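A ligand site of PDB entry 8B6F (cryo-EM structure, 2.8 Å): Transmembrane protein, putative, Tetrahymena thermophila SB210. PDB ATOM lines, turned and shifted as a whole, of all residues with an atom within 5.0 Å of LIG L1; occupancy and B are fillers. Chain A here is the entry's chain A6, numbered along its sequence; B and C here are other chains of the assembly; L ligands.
The side-chain hydroxyl (OH) of Tyr 145 sits at hydrogen-bond distance from an oxygen (O7) of LIG L1 (2.7 Å). The guanidinium group (NH2) of Arg 266 of chain B lies within salt-bridge range of an oxygen (O3) of LIG L1, 2.8 Å away. The guanidinium group (NE) of Arg 158 is in hydrogen-bond range of an oxygen (O6) of LIG L1 (3.3 Å).
NH2 of Arg 158 is in hydrogen-bond range of OH of Tyr 145, 3.0 Å away. The side-chain carboxylate (OE1) of Glu 155 lies within salt-bridge range of the guanidinium group (NH2) of Arg 266 of chain B (3.6 Å). The side-chain hydroxyl of Tyr 154 sits close to the side-chain hydroxyl of Tyr 116, at 3.5 Å. OE1 of Glu 155 is in salt-bridge range of NH1 of Arg 158 (3.4 Å). OE1 of Glu 120 sits at hydrogen-bond distance from N of Phe 181 (3.4 Å). The side-chain carboxylate (OE2) of Glu 120 lies within salt-bridge range of the guanidinium group (NE) of Arg 117, 2.9 Å away.
Merely in contact with LIG L1: Tyr 116, Arg 117, Glu 120, Leu 124, Ala 138, Ala 141, Ile 142, Tyr 154, Ala 180, Phe 181 and Phe 263 of chain B. Hydrophobic or aromatic side chains that line LIG L1: Leu 124, Ala 138, Ile 142, Tyr 145, Tyr 154, Ala 180, Phe 181 and Phe 263 of chain B. Of the 19 residues printed, 14 come within 4 Å of LIG L1. The nearest printed residue that does not touch LIG L1 is Leu 264 of chain B (4.3 Å).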
ATOM      1  N   TYR A 116     -23.238   5.838  -5.935  1.00  0.00           N
ATOM      2  CA  TYR A 116     -23.389   4.581  -5.205  1.00  0.00           C
ATOM      3  C   TYR A 116     -23.600   3.416  -6.156  1.00  0.00           C
ATOM      4  O   TYR A 116     -22.959   2.366  -6.016  1.00  0.00           O
ATOM      5  CB  TYR A 116     -24.545   4.679  -4.217  1.00  0.00           C
ATOM      6  CG  TYR A 116     -24.696   3.446  -3.353  1.00  0.00           C
ATOM      7  CD1 TYR A 116     -25.450   2.364  -3.775  1.00  0.00           C
ATOM      8  CD2 TYR A 116     -24.080   3.379  -2.106  1.00  0.00           C
ATOM      9  CE1 TYR A 116     -25.588   1.245  -2.980  1.00  0.00           C
ATOM     10  CE2 TYR A 116     -24.205   2.261  -1.313  1.00  0.00           C
ATOM     11  CZ  TYR A 116     -24.962   1.193  -1.746  1.00  0.00           C
ATOM     12  OH  TYR A 116     -25.095   0.086  -0.955  1.00  0.00           O
ATOM     13  N   ARG A 117     -24.502   3.569  -7.134  1.00  0.00           N
ATOM     14  CA  ARG A 117     -24.747   2.482  -8.072  1.00  0.00           C
ATOM     15  C   ARG A 117     -23.570   2.265  -9.007  1.00  0.00           C
ATOM     16  O   ARG A 117     -23.441   1.176  -9.581  1.00  0.00           O
ATOM     17  CB  ARG A 117     -26.010   2.770  -8.894  1.00  0.00           C
ATOM     18  CG  ARG A 117     -27.278   2.975  -8.078  1.00  0.00           C
ATOM     19  CD  ARG A 117     -27.596   1.780  -7.193  1.00  0.00           C
ATOM     20  NE  ARG A 117     -27.793   0.548  -7.941  1.00  0.00           N
ATOM     21  CZ  ARG A 117     -28.950   0.133  -8.434  1.00  0.00           C
ATOM     22  NH1 ARG A 117     -30.058   0.853  -8.301  1.00  0.00           N
ATOM     23  NH2 ARG A 117     -29.011  -1.033  -9.065  1.00  0.00           N
ATOM     24  N   GLU A 120     -21.049  -0.806  -8.544  1.00  0.00           N
ATOM     25  CA  GLU A 120     -21.257  -2.132  -9.115  1.00  0.00           C
ATOM     26  C   GLU A 120     -20.377  -2.389 -10.322  1.00  0.00           C
ATOM     27  O   GLU A 120     -20.275  -3.540 -10.758  1.00  0.00           O
ATOM     28  CB  GLU A 120     -22.726  -2.306  -9.484  1.00  0.00           C
ATOM     29  CG  GLU A 120     -23.681  -2.101  -8.321  1.00  0.00           C
ATOM     30  CD  GLU A 120     -25.135  -2.219  -8.738  1.00  0.00           C
ATOM     31  OE1 GLU A 120     -25.405  -2.752  -9.832  1.00  0.00           O
ATOM     32  OE2 GLU A 120     -26.017  -1.775  -7.965  1.00  0.00           O
ATOM     33  N   LEU A 124     -17.628  -4.830  -7.803  1.00  0.00           N
ATOM     34  CA  LEU A 124     -18.109  -6.176  -8.092  1.00  0.00           C
ATOM     35  C   LEU A 124     -17.122  -6.956  -8.949  1.00  0.00           C
ATOM     36  O   LEU A 124     -16.644  -8.016  -8.509  1.00  0.00           O
ATOM     37  CB  LEU A 124     -19.515  -6.110  -8.707  1.00  0.00           C
ATOM     38  CG  LEU A 124     -20.018  -7.353  -9.434  1.00  0.00           C
ATOM     39  CD1 LEU A 124     -20.143  -8.521  -8.467  1.00  0.00           C
ATOM     40  CD2 LEU A 124     -21.341  -7.068 -10.110  1.00  0.00           C
ATOM     41  N   ALA A 138     -20.318 -13.312  -1.831  1.00  0.00           N
ATOM     42  CA  ALA A 138     -21.700 -13.289  -2.291  1.00  0.00           C
ATOM     43  C   ALA A 138     -22.659 -13.770  -1.211  1.00  0.00           C
ATOM     44  O   ALA A 138     -23.737 -13.197  -1.028  1.00  0.00           O
ATOM     45  CB  ALA A 138     -21.850 -14.146  -3.544  1.00  0.00           C
ATOM     46  N   ALA A 141     -23.118 -11.006   1.133  1.00  0.00           N
ATOM     47  CA  ALA A 141     -23.809  -9.855   0.560  1.00  0.00           C
ATOM     48  C   ALA A 141     -25.304 -10.104   0.414  1.00  0.00           C
ATOM     49  O   ALA A 141     -26.110  -9.178   0.572  1.00  0.00           O
ATOM     50  CB  ALA A 141     -23.195  -9.501  -0.791  1.00  0.00           C
ATOM     51  N   ILE A 142     -25.700 -11.334   0.095  1.00  0.00           N
ATOM     52  CA  ILE A 142     -27.097 -11.652  -0.194  1.00  0.00           C
ATOM     53  C   ILE A 142     -27.974 -11.216   0.972  1.00  0.00           C
ATOM     54  O   ILE A 142     -28.826 -10.335   0.805  1.00  0.00           O
ATOM     55  CB  ILE A 142     -27.280 -13.143  -0.509  1.00  0.00           C
ATOM     56  CG1 ILE A 142     -26.754 -13.453  -1.920  1.00  0.00           C
ATOM     57  CG2 ILE A 142     -28.746 -13.562  -0.349  1.00  0.00           C
ATOM     58  CD1 ILE A 142     -27.657 -12.976  -3.048  1.00  0.00           C
ATOM     59  N   SER A 144     -27.218  -9.345   3.443  1.00  0.00           N
ATOM     60  CA  SER A 144     -27.007  -7.914   3.645  1.00  0.00           C
ATOM     61  C   SER A 144     -27.868  -7.100   2.693  1.00  0.00           C
ATOM     62  O   SER A 144     -28.458  -6.092   3.106  1.00  0.00           O
ATOM     63  CB  SER A 144     -25.525  -7.577   3.444  1.00  0.00           C
ATOM     64  OG  SER A 144     -24.718  -8.215   4.427  1.00  0.00           O
ATOM     65  N   TYR A 145     -27.955  -7.516   1.437  1.00  0.00           N
ATOM     66  CA  TYR A 145     -28.830  -6.831   0.496  1.00  0.00           C
ATOM     67  C   TYR A 145     -30.291  -6.928   0.916  1.00  0.00           C
ATOM     68  O   TYR A 145     -31.025  -5.940   0.904  1.00  0.00           O
ATOM     69  CB  TYR A 145     -28.647  -7.399  -0.910  1.00  0.00           C
ATOM     70  CG  TYR A 145     -29.726  -6.948  -1.866  1.00  0.00           C
ATOM     71  CD1 TYR A 145     -29.679  -5.704  -2.459  1.00  0.00           C
ATOM     72  CD2 TYR A 145     -30.794  -7.785  -2.179  1.00  0.00           C
ATOM     73  CE1 TYR A 145     -30.661  -5.283  -3.332  1.00  0.00           C
ATOM     74  CE2 TYR A 145     -31.781  -7.377  -3.046  1.00  0.00           C
ATOM     75  CZ  TYR A 145     -31.710  -6.126  -3.620  1.00  0.00           C
ATOM     76  OH  TYR A 145     -32.691  -5.715  -4.495  1.00  0.00           O
ATOM     77  N   PHE A 149     -30.129  -3.083   3.335  1.00  0.00           N
ATOM     78  CA  PHE A 149     -29.527  -2.455   2.153  1.00  0.00           C
ATOM     79  C   PHE A 149     -30.531  -2.256   1.029  1.00  0.00           C
ATOM     80  O   PHE A 149     -30.608  -1.161   0.465  1.00  0.00           O
ATOM     81  CB  PHE A 149     -28.344  -3.284   1.646  1.00  0.00           C
ATOM     82  CG  PHE A 149     -27.045  -2.957   2.324  1.00  0.00           C
ATOM     83  CD1 PHE A 149     -26.309  -1.848   1.920  1.00  0.00           C
ATOM     84  CD2 PHE A 149     -26.549  -3.745   3.343  1.00  0.00           C
ATOM     85  CE1 PHE A 149     -25.114  -1.538   2.532  1.00  0.00           C
ATOM     86  CE2 PHE A 149     -25.354  -3.435   3.956  1.00  0.00           C
ATOM     87  CZ  PHE A 149     -24.640  -2.326   3.549  1.00  0.00           C
ATOM     88  N   TYR A 154     -31.555   0.766  -2.391  1.00  0.00           N
ATOM     89  CA  TYR A 154     -31.734   0.294  -3.756  1.00  0.00           C
ATOM     90  C   TYR A 154     -33.147   0.539  -4.268  1.00  0.00           C
ATOM     91  O   TYR A 154     -33.335   1.054  -5.373  1.00  0.00           O
ATOM     92  CB  TYR A 154     -31.373  -1.192  -3.851  1.00  0.00           C
ATOM     93  CG  TYR A 154     -29.889  -1.448  -3.760  1.00  0.00           C
ATOM     94  CD1 TYR A 154     -29.064  -1.240  -4.857  1.00  0.00           C
ATOM     95  CD2 TYR A 154     -29.319  -1.903  -2.581  1.00  0.00           C
ATOM     96  CE1 TYR A 154     -27.709  -1.466  -4.784  1.00  0.00           C
ATOM     97  CE2 TYR A 154     -27.961  -2.133  -2.495  1.00  0.00           C
ATOM     98  CZ  TYR A 154     -27.161  -1.912  -3.606  1.00  0.00           C
ATOM     99  OH  TYR A 154     -25.812  -2.140  -3.525  1.00  0.00           O
ATOM    100  N   GLU A 155     -34.155   0.189  -3.471  1.00  0.00           N
ATOM    101  CA  GLU A 155     -35.532   0.415  -3.913  1.00  0.00           C
ATOM    102  C   GLU A 155     -35.820   1.900  -4.058  1.00  0.00           C
ATOM    103  O   GLU A 155     -36.498   2.317  -5.008  1.00  0.00           O
ATOM    104  CB  GLU A 155     -36.516  -0.233  -2.943  1.00  0.00           C
ATOM    105  CG  GLU A 155     -37.968  -0.099  -3.365  1.00  0.00           C
ATOM    106  CD  GLU A 155     -38.246  -0.714  -4.720  1.00  0.00           C
ATOM    107  OE1 GLU A 155     -37.447  -1.559  -5.161  1.00  0.00           O
ATOM    108  OE2 GLU A 155     -39.271  -0.358  -5.339  1.00  0.00           O
ATOM    109  N   ARG A 158     -34.364   2.928  -7.292  1.00  0.00           N
ATOM    110  CA  ARG A 158     -35.152   2.454  -8.429  1.00  0.00           C
ATOM    111  C   ARG A 158     -36.369   3.327  -8.665  1.00  0.00           C
ATOM    112  O   ARG A 158     -36.730   3.617  -9.812  1.00  0.00           O
ATOM    113  CB  ARG A 158     -35.586   1.001  -8.189  1.00  0.00           C
ATOM    114  CG  ARG A 158     -34.458  -0.010  -8.249  1.00  0.00           C
ATOM    115  CD  ARG A 158     -34.994  -1.426  -8.195  1.00  0.00           C
ATOM    116  NE  ARG A 158     -33.941  -2.408  -7.970  1.00  0.00           N
ATOM    117  CZ  ARG A 158     -33.571  -2.865  -6.781  1.00  0.00           C
ATOM    118  NH1 ARG A 158     -34.164  -2.473  -5.670  1.00  0.00           N
ATOM    119  NH2 ARG A 158     -32.583  -3.754  -6.712  1.00  0.00           N
ATOM    120  N   ALA A 180     -29.027  -0.156 -13.005  1.00  0.00           N
ATOM    121  CA  ALA A 180     -27.897  -0.922 -12.505  1.00  0.00           C
ATOM    122  C   ALA A 180     -26.597  -0.352 -13.038  1.00  0.00           C
ATOM    123  O   ALA A 180     -26.496   0.059 -14.201  1.00  0.00           O
ATOM    124  CB  ALA A 180     -28.032  -2.386 -12.905  1.00  0.00           C
ATOM    125  N   PHE A 181     -25.577  -0.318 -12.183  1.00  0.00           N
ATOM    126  CA  PHE A 181     -24.246   0.172 -12.542  1.00  0.00           C
ATOM    127  C   PHE A 181     -24.250   1.653 -12.880  1.00  0.00           C
ATOM    128  O   PHE A 181     -23.322   2.143 -13.524  1.00  0.00           O
ATOM    129  CB  PHE A 181     -23.664  -0.643 -13.708  1.00  0.00           C
ATOM    130  CG  PHE A 181     -23.688  -2.122 -13.491  1.00  0.00           C
ATOM    131  CD1 PHE A 181     -22.713  -2.732 -12.722  1.00  0.00           C
ATOM    132  CD2 PHE A 181     -24.672  -2.901 -14.067  1.00  0.00           C
ATOM    133  CE1 PHE A 181     -22.723  -4.102 -12.523  1.00  0.00           C
ATOM    134  CE2 PHE A 181     -24.696  -4.272 -13.865  1.00  0.00           C
ATOM    135  CZ  PHE A 181     -23.721  -4.872 -13.093  1.00  0.00           C
ATOM    136  N   PHE B 263     -37.005  -6.945 -16.359  1.00  0.00           N
ATOM    137  CA  PHE B 263     -36.145  -7.053 -15.181  1.00  0.00           C
ATOM    138  C   PHE B 263     -35.274  -5.805 -15.029  1.00  0.00           C
ATOM    139  O   PHE B 263     -35.167  -5.238 -13.937  1.00  0.00           O
ATOM    140  CB  PHE B 263     -35.275  -8.304 -15.285  1.00  0.00           C
ATOM    141  CG  PHE B 263     -34.314  -8.469 -14.143  1.00  0.00           C
ATOM    142  CD1 PHE B 263     -34.742  -8.974 -12.925  1.00  0.00           C
ATOM    143  CD2 PHE B 263     -32.980  -8.125 -14.282  1.00  0.00           C
ATOM    144  CE1 PHE B 263     -33.863  -9.137 -11.878  1.00  0.00           C
ATOM    145  CE2 PHE B 263     -32.088  -8.287 -13.238  1.00  0.00           C
ATOM    146  CZ  PHE B 263     -32.532  -8.789 -12.030  1.00  0.00           C
ATOM    147  N   LEU B 264     -34.651  -5.369 -16.119  1.00  0.00           N
ATOM    148  CA  LEU B 264     -33.812  -4.179 -16.133  1.00  0.00           C
ATOM    149  C   LEU B 264     -34.566  -3.066 -16.839  1.00  0.00           C
ATOM    150  O   LEU B 264     -35.062  -3.250 -17.955  1.00  0.00           O
ATOM    151  CB  LEU B 264     -32.480  -4.464 -16.842  1.00  0.00           C
ATOM    152  CG  LEU B 264     -31.385  -3.408 -16.706  1.00  0.00           C
ATOM    153  CD1 LEU B 264     -30.862  -3.375 -15.278  1.00  0.00           C
ATOM    154  CD2 LEU B 264     -30.260  -3.688 -17.685  1.00  0.00           C
ATOM    155  N   ARG B 266     -37.373  -1.977 -15.989  1.00  0.00           N
ATOM    156  CA  ARG B 266     -38.784  -2.150 -15.660  1.00  0.00           C
ATOM    157  C   ARG B 266     -39.684  -1.550 -16.746  1.00  0.00           C
ATOM    158  O   ARG B 266     -40.437  -0.610 -16.520  1.00  0.00           O
ATOM    159  CB  ARG B 266     -39.103  -1.535 -14.296  1.00  0.00           C
ATOM    160  CG  ARG B 266     -38.470  -2.267 -13.124  1.00  0.00           C
ATOM    161  CD  ARG B 266     -38.877  -1.633 -11.805  1.00  0.00           C
ATOM    162  NE  ARG B 266     -38.398  -2.405 -10.665  1.00  0.00           N
ATOM    163  CZ  ARG B 266     -38.616  -2.083  -9.388  1.00  0.00           C
ATOM    164  NH1 ARG B 266     -39.302  -1.000  -9.069  1.00  0.00           N
ATOM    165  NH2 ARG B 266     -38.139  -2.865  -8.430  1.00  0.00           N
ATOM    166  N   ILE C 736     -16.810   2.553   1.434  1.00  0.00           N
ATOM    167  CA  ILE C 736     -16.765   1.259   0.760  1.00  0.00           C
ATOM    168  C   ILE C 736     -15.689   1.251  -0.305  1.00  0.00           C
ATOM    169  O   ILE C 736     -14.851   0.339  -0.361  1.00  0.00           O
ATOM    170  CB  ILE C 736     -18.142   0.925   0.164  1.00  0.00           C
ATOM    171  CG1 ILE C 736     -19.196   0.795   1.277  1.00  0.00           C
ATOM    172  CG2 ILE C 736     -18.081  -0.357  -0.659  1.00  0.00           C
ATOM    173  CD1 ILE C 736     -20.620   0.661   0.775  1.00  0.00           C
HETATM  174  P1  LIG L   1     -37.950  -6.555  -8.240  1.00  0.00           P
HETATM  175  O1  LIG L   1     -39.376  -6.891  -8.580  1.00  0.00           O
HETATM  176  O2  LIG L   1     -37.239  -7.731  -7.610  1.00  0.00           O
HETATM  177  O3  LIG L   1     -38.011  -5.386  -7.276  1.00  0.00           O
HETATM  178  O4  LIG L   1     -37.181  -6.052  -9.610  1.00  0.00           O
HETATM  179  C1  LIG L   1     -36.177  -6.854 -10.133  1.00  0.00           C
HETATM  180  C2  LIG L   1     -34.824  -6.340  -9.661  1.00  0.00           C
HETATM  181  C3  LIG L   1     -34.454  -5.033 -10.347  1.00  0.00           C
HETATM  182  O5  LIG L   1     -34.878  -6.140  -8.257  1.00  0.00           O
HETATM  183  O6  LIG L   1     -33.101  -4.842 -10.054  1.00  0.00           O
HETATM  184  C4  LIG L   1     -34.306  -7.081  -7.385  1.00  0.00           C
HETATM  185  O7  LIG L   1     -34.386  -6.898  -6.219  1.00  0.00           O
HETATM  186  C5  LIG L   1     -33.588  -8.326  -7.897  1.00  0.00           C
HETATM  187  C6  LIG L   1     -32.129  -8.028  -8.254  1.00  0.00           C
HETATM  188  C7  LIG L   1     -31.297  -7.584  -7.045  1.00  0.00           C
HETATM  189  C8  LIG L   1     -29.920  -7.048  -7.446  1.00  0.00           C
HETATM  190  C9  LIG L   1     -29.226  -6.333  -6.298  1.00  0.00           C
HETATM  191  C10 LIG L   1     -27.870  -5.753  -6.713  1.00  0.00           C
HETATM  192  C11 LIG L   1     -27.131  -5.027  -5.594  1.00  0.00           C
HETATM  193  C12 LIG L   1     -26.485  -6.017  -4.609  1.00  0.00           C
HETATM  194  C13 LIG L   1     -25.927  -5.330  -3.351  1.00  0.00           C
HETATM  195  C14 LIG L   1     -25.246  -6.333  -2.421  1.00  0.00           C
HETATM  196  C15 LIG L   1     -25.051  -5.790  -1.010  1.00  0.00           C
HETATM  197  C16 LIG L   1     -24.186  -4.525  -0.919  1.00  0.00           C
HETATM  198  C17 LIG L   1     -22.750  -4.753  -1.371  1.00  0.00           C
HETATM  199  C18 LIG L   1     -21.866  -3.533  -1.117  1.00  0.00           C
HETATM  200  C19 LIG L   1     -22.304  -2.311  -1.932  1.00  0.00           C
HETATM  201  C20 LIG L   1     -32.394  -3.864 -10.735  1.00  0.00           C
HETATM  202  O8  LIG L   1     -32.912  -3.110 -11.491  1.00  0.00           O
HETATM  203  C21 LIG L   1     -30.887  -3.825 -10.471  1.00  0.00           C
HETATM  204  C22 LIG L   1     -30.155  -4.906 -11.262  1.00  0.00           C
HETATM  205  C23 LIG L   1     -28.701  -4.999 -10.799  1.00  0.00           C
HETATM  206  C24 LIG L   1     -27.890  -5.917 -11.711  1.00  0.00           C
HETATM  207  C25 LIG L   1     -26.410  -5.950 -11.311  1.00  0.00           C
HETATM  208  C26 LIG L   1     -26.199  -6.538  -9.909  1.00  0.00           C
HETATM  209  C27 LIG L   1     -24.708  -6.600  -9.549  1.00  0.00           C
HETATM  210  C28 LIG L   1     -24.447  -7.284  -8.207  1.00  0.00           C
HETATM  211  C29 LIG L   1     -24.662  -8.805  -8.276  1.00  0.00           C
HETATM  212  C30 LIG L   1     -24.492  -9.461  -6.900  1.00  0.00           C
HETATM  213  C31 LIG L   1     -24.682 -10.976  -6.988  1.00  0.00           C
HETATM  214  C32 LIG L   1     -24.757 -11.616  -5.602  1.00  0.00           C
HETATM  215  C33 LIG L   1     -24.822 -13.147  -5.645  1.00  0.00           C
HETATM  216  C34 LIG L   1     -25.999 -13.674  -6.478  1.00  0.00           C
HETATM  217  C35 LIG L   1     -26.076 -15.196  -6.375  1.00  0.00           C
HETATM  218  O1  LG2 L   2      -9.069 -13.219   0.114  1.00  0.00           O
HETATM  219  P1  LG2 L   2     -10.404 -13.113   0.826  1.00  0.00           P
HETATM  220  O2  LG2 L   2     -11.474 -14.122   0.496  1.00  0.00           O
HETATM  221  O3  LG2 L   2     -10.166 -13.130   2.455  1.00  0.00           O
HETATM  222  C1  LG2 L   2      -9.717 -14.297   3.081  1.00  0.00           C
HETATM  223  C2  LG2 L   2     -10.998 -14.996   3.522  1.00  0.00           C
HETATM  224  N1  LG2 L   2     -11.531 -14.600   4.816  1.00  0.00           N
HETATM  225  C3  LG2 L   2     -12.857 -15.118   4.981  1.00  0.00           C
HETATM  226  C4  LG2 L   2     -10.681 -15.120   5.868  1.00  0.00           C
HETATM  227  C5  LG2 L   2     -11.577 -13.153   4.919  1.00  0.00           C
HETATM  228  O4  LG2 L   2     -11.045 -11.596   0.583  1.00  0.00           O
HETATM  229  C6  LG2 L   2     -12.318 -11.333   1.162  1.00  0.00           C
HETATM  230  C7  LG2 L   2     -12.266 -10.015   1.949  1.00  0.00           C
HETATM  231  O5  LG2 L   2     -13.427  -9.284   1.707  1.00  0.00           O
HETATM  232  C8  LG2 L   2     -14.619  -9.731   2.304  1.00  0.00           C
HETATM  233  O6  LG2 L   2     -14.613 -10.554   3.145  1.00  0.00           O
HETATM  234  C9  LG2 L   2     -15.948  -9.124   1.778  1.00  0.00           C
HETATM  235  C10 LG2 L   2     -17.172  -9.895   2.300  1.00  0.00           C
HETATM  236  C11 LG2 L   2     -18.418  -9.491   1.514  1.00  0.00           C
HETATM  237  C12 LG2 L   2     -18.949  -8.098   1.903  1.00  0.00           C
HETATM  238  C13 LG2 L   2     -20.370  -7.915   1.352  1.00  0.00           C
HETATM  239  C14 LG2 L   2     -20.969  -6.528   1.641  1.00  0.00           C
HETATM  240  C15 LG2 L   2     -20.969  -6.186   3.141  1.00  0.00           C
HETATM  241  C16 LG2 L   2     -19.963  -5.054   3.465  1.00  0.00           C
HETATM  242  C17 LG2 L   2     -20.475  -3.694   2.958  1.00  0.00           C
HETATM  243  C18 LG2 L   2     -19.369  -2.849   2.264  1.00  0.00           C
HETATM  244  C19 LG2 L   2     -18.364  -2.199   3.256  1.00  0.00           C
HETATM  245  C20 LG2 L   2     -17.433  -3.217   3.951  1.00  0.00           C
HETATM  246  C21 LG2 L   2     -16.279  -2.494   4.641  1.00  0.00           C
HETATM  247  C22 LG2 L   2     -15.345  -3.481   5.337  1.00  0.00           C
HETATM  248  C23 LG2 L   2     -14.200  -2.747   6.025  1.00  0.00           C
HETATM  249  C24 LG2 L   2     -13.255  -3.675   6.772  1.00  0.00           C
HETATM  250  C25 LG2 L   2     -13.988  -4.451   7.866  1.00  0.00           C
HETATM  251  C26 LG2 L   2     -11.133  -9.187   1.394  1.00  0.00           C
HETATM  252  O7  LG2 L   2     -11.497  -7.825   1.485  1.00  0.00           O
HETATM  253  C27 LG2 L   2     -11.455  -7.238   2.790  1.00  0.00           C
HETATM  254  O8  LG2 L   2     -11.500  -7.884   3.765  1.00  0.00           O
HETATM  255  C28 LG2 L   2     -11.347  -5.712   2.786  1.00  0.00           C
HETATM  256  C29 LG2 L   2     -12.729  -5.032   2.650  1.00  0.00           C
HETATM  257  C30 LG2 L   2     -13.401  -5.368   1.310  1.00  0.00           C
HETATM  258  C31 LG2 L   2     -14.822  -4.790   1.266  1.00  0.00           C
HETATM  259  C32 LG2 L   2     -15.561  -5.201  -0.005  1.00  0.00           C
HETATM  260  C33 LG2 L   2     -16.993  -4.637   0.001  1.00  0.00           C
HETATM  261  C34 LG2 L   2     -17.703  -4.873  -1.333  1.00  0.00           C
HETATM  262  C35 LG2 L   2     -18.420  -6.238  -1.377  1.00  0.00           C
HETATM  263  C36 LG2 L   2     -19.318  -6.319  -2.630  1.00  0.00           C
HETATM  264  C37 LG2 L   2     -20.209  -7.572  -2.660  1.00  0.00           C
HETATM  265  C38 LG2 L   2     -19.438  -8.907  -2.595  1.00  0.00           C
HETATM  266  C39 LG2 L   2     -18.473  -9.141  -3.760  1.00  0.00           C
HETATM  267  C40 LG2 L   2     -19.184  -9.476  -5.076  1.00  0.00           C
HETATM  268  C41 LG2 L   2     -19.357 -10.982  -5.263  1.00  0.00           C
HETATM  269  C42 LG2 L   2     -19.805 -11.306  -6.681  1.00  0.00           C
HETATM  270  C43 LG2 L   2     -20.010 -12.808  -6.927  1.00  0.00           C
HETATM  271  C44 LG2 L   2     -18.712 -13.604  -6.761  1.00  0.00           C
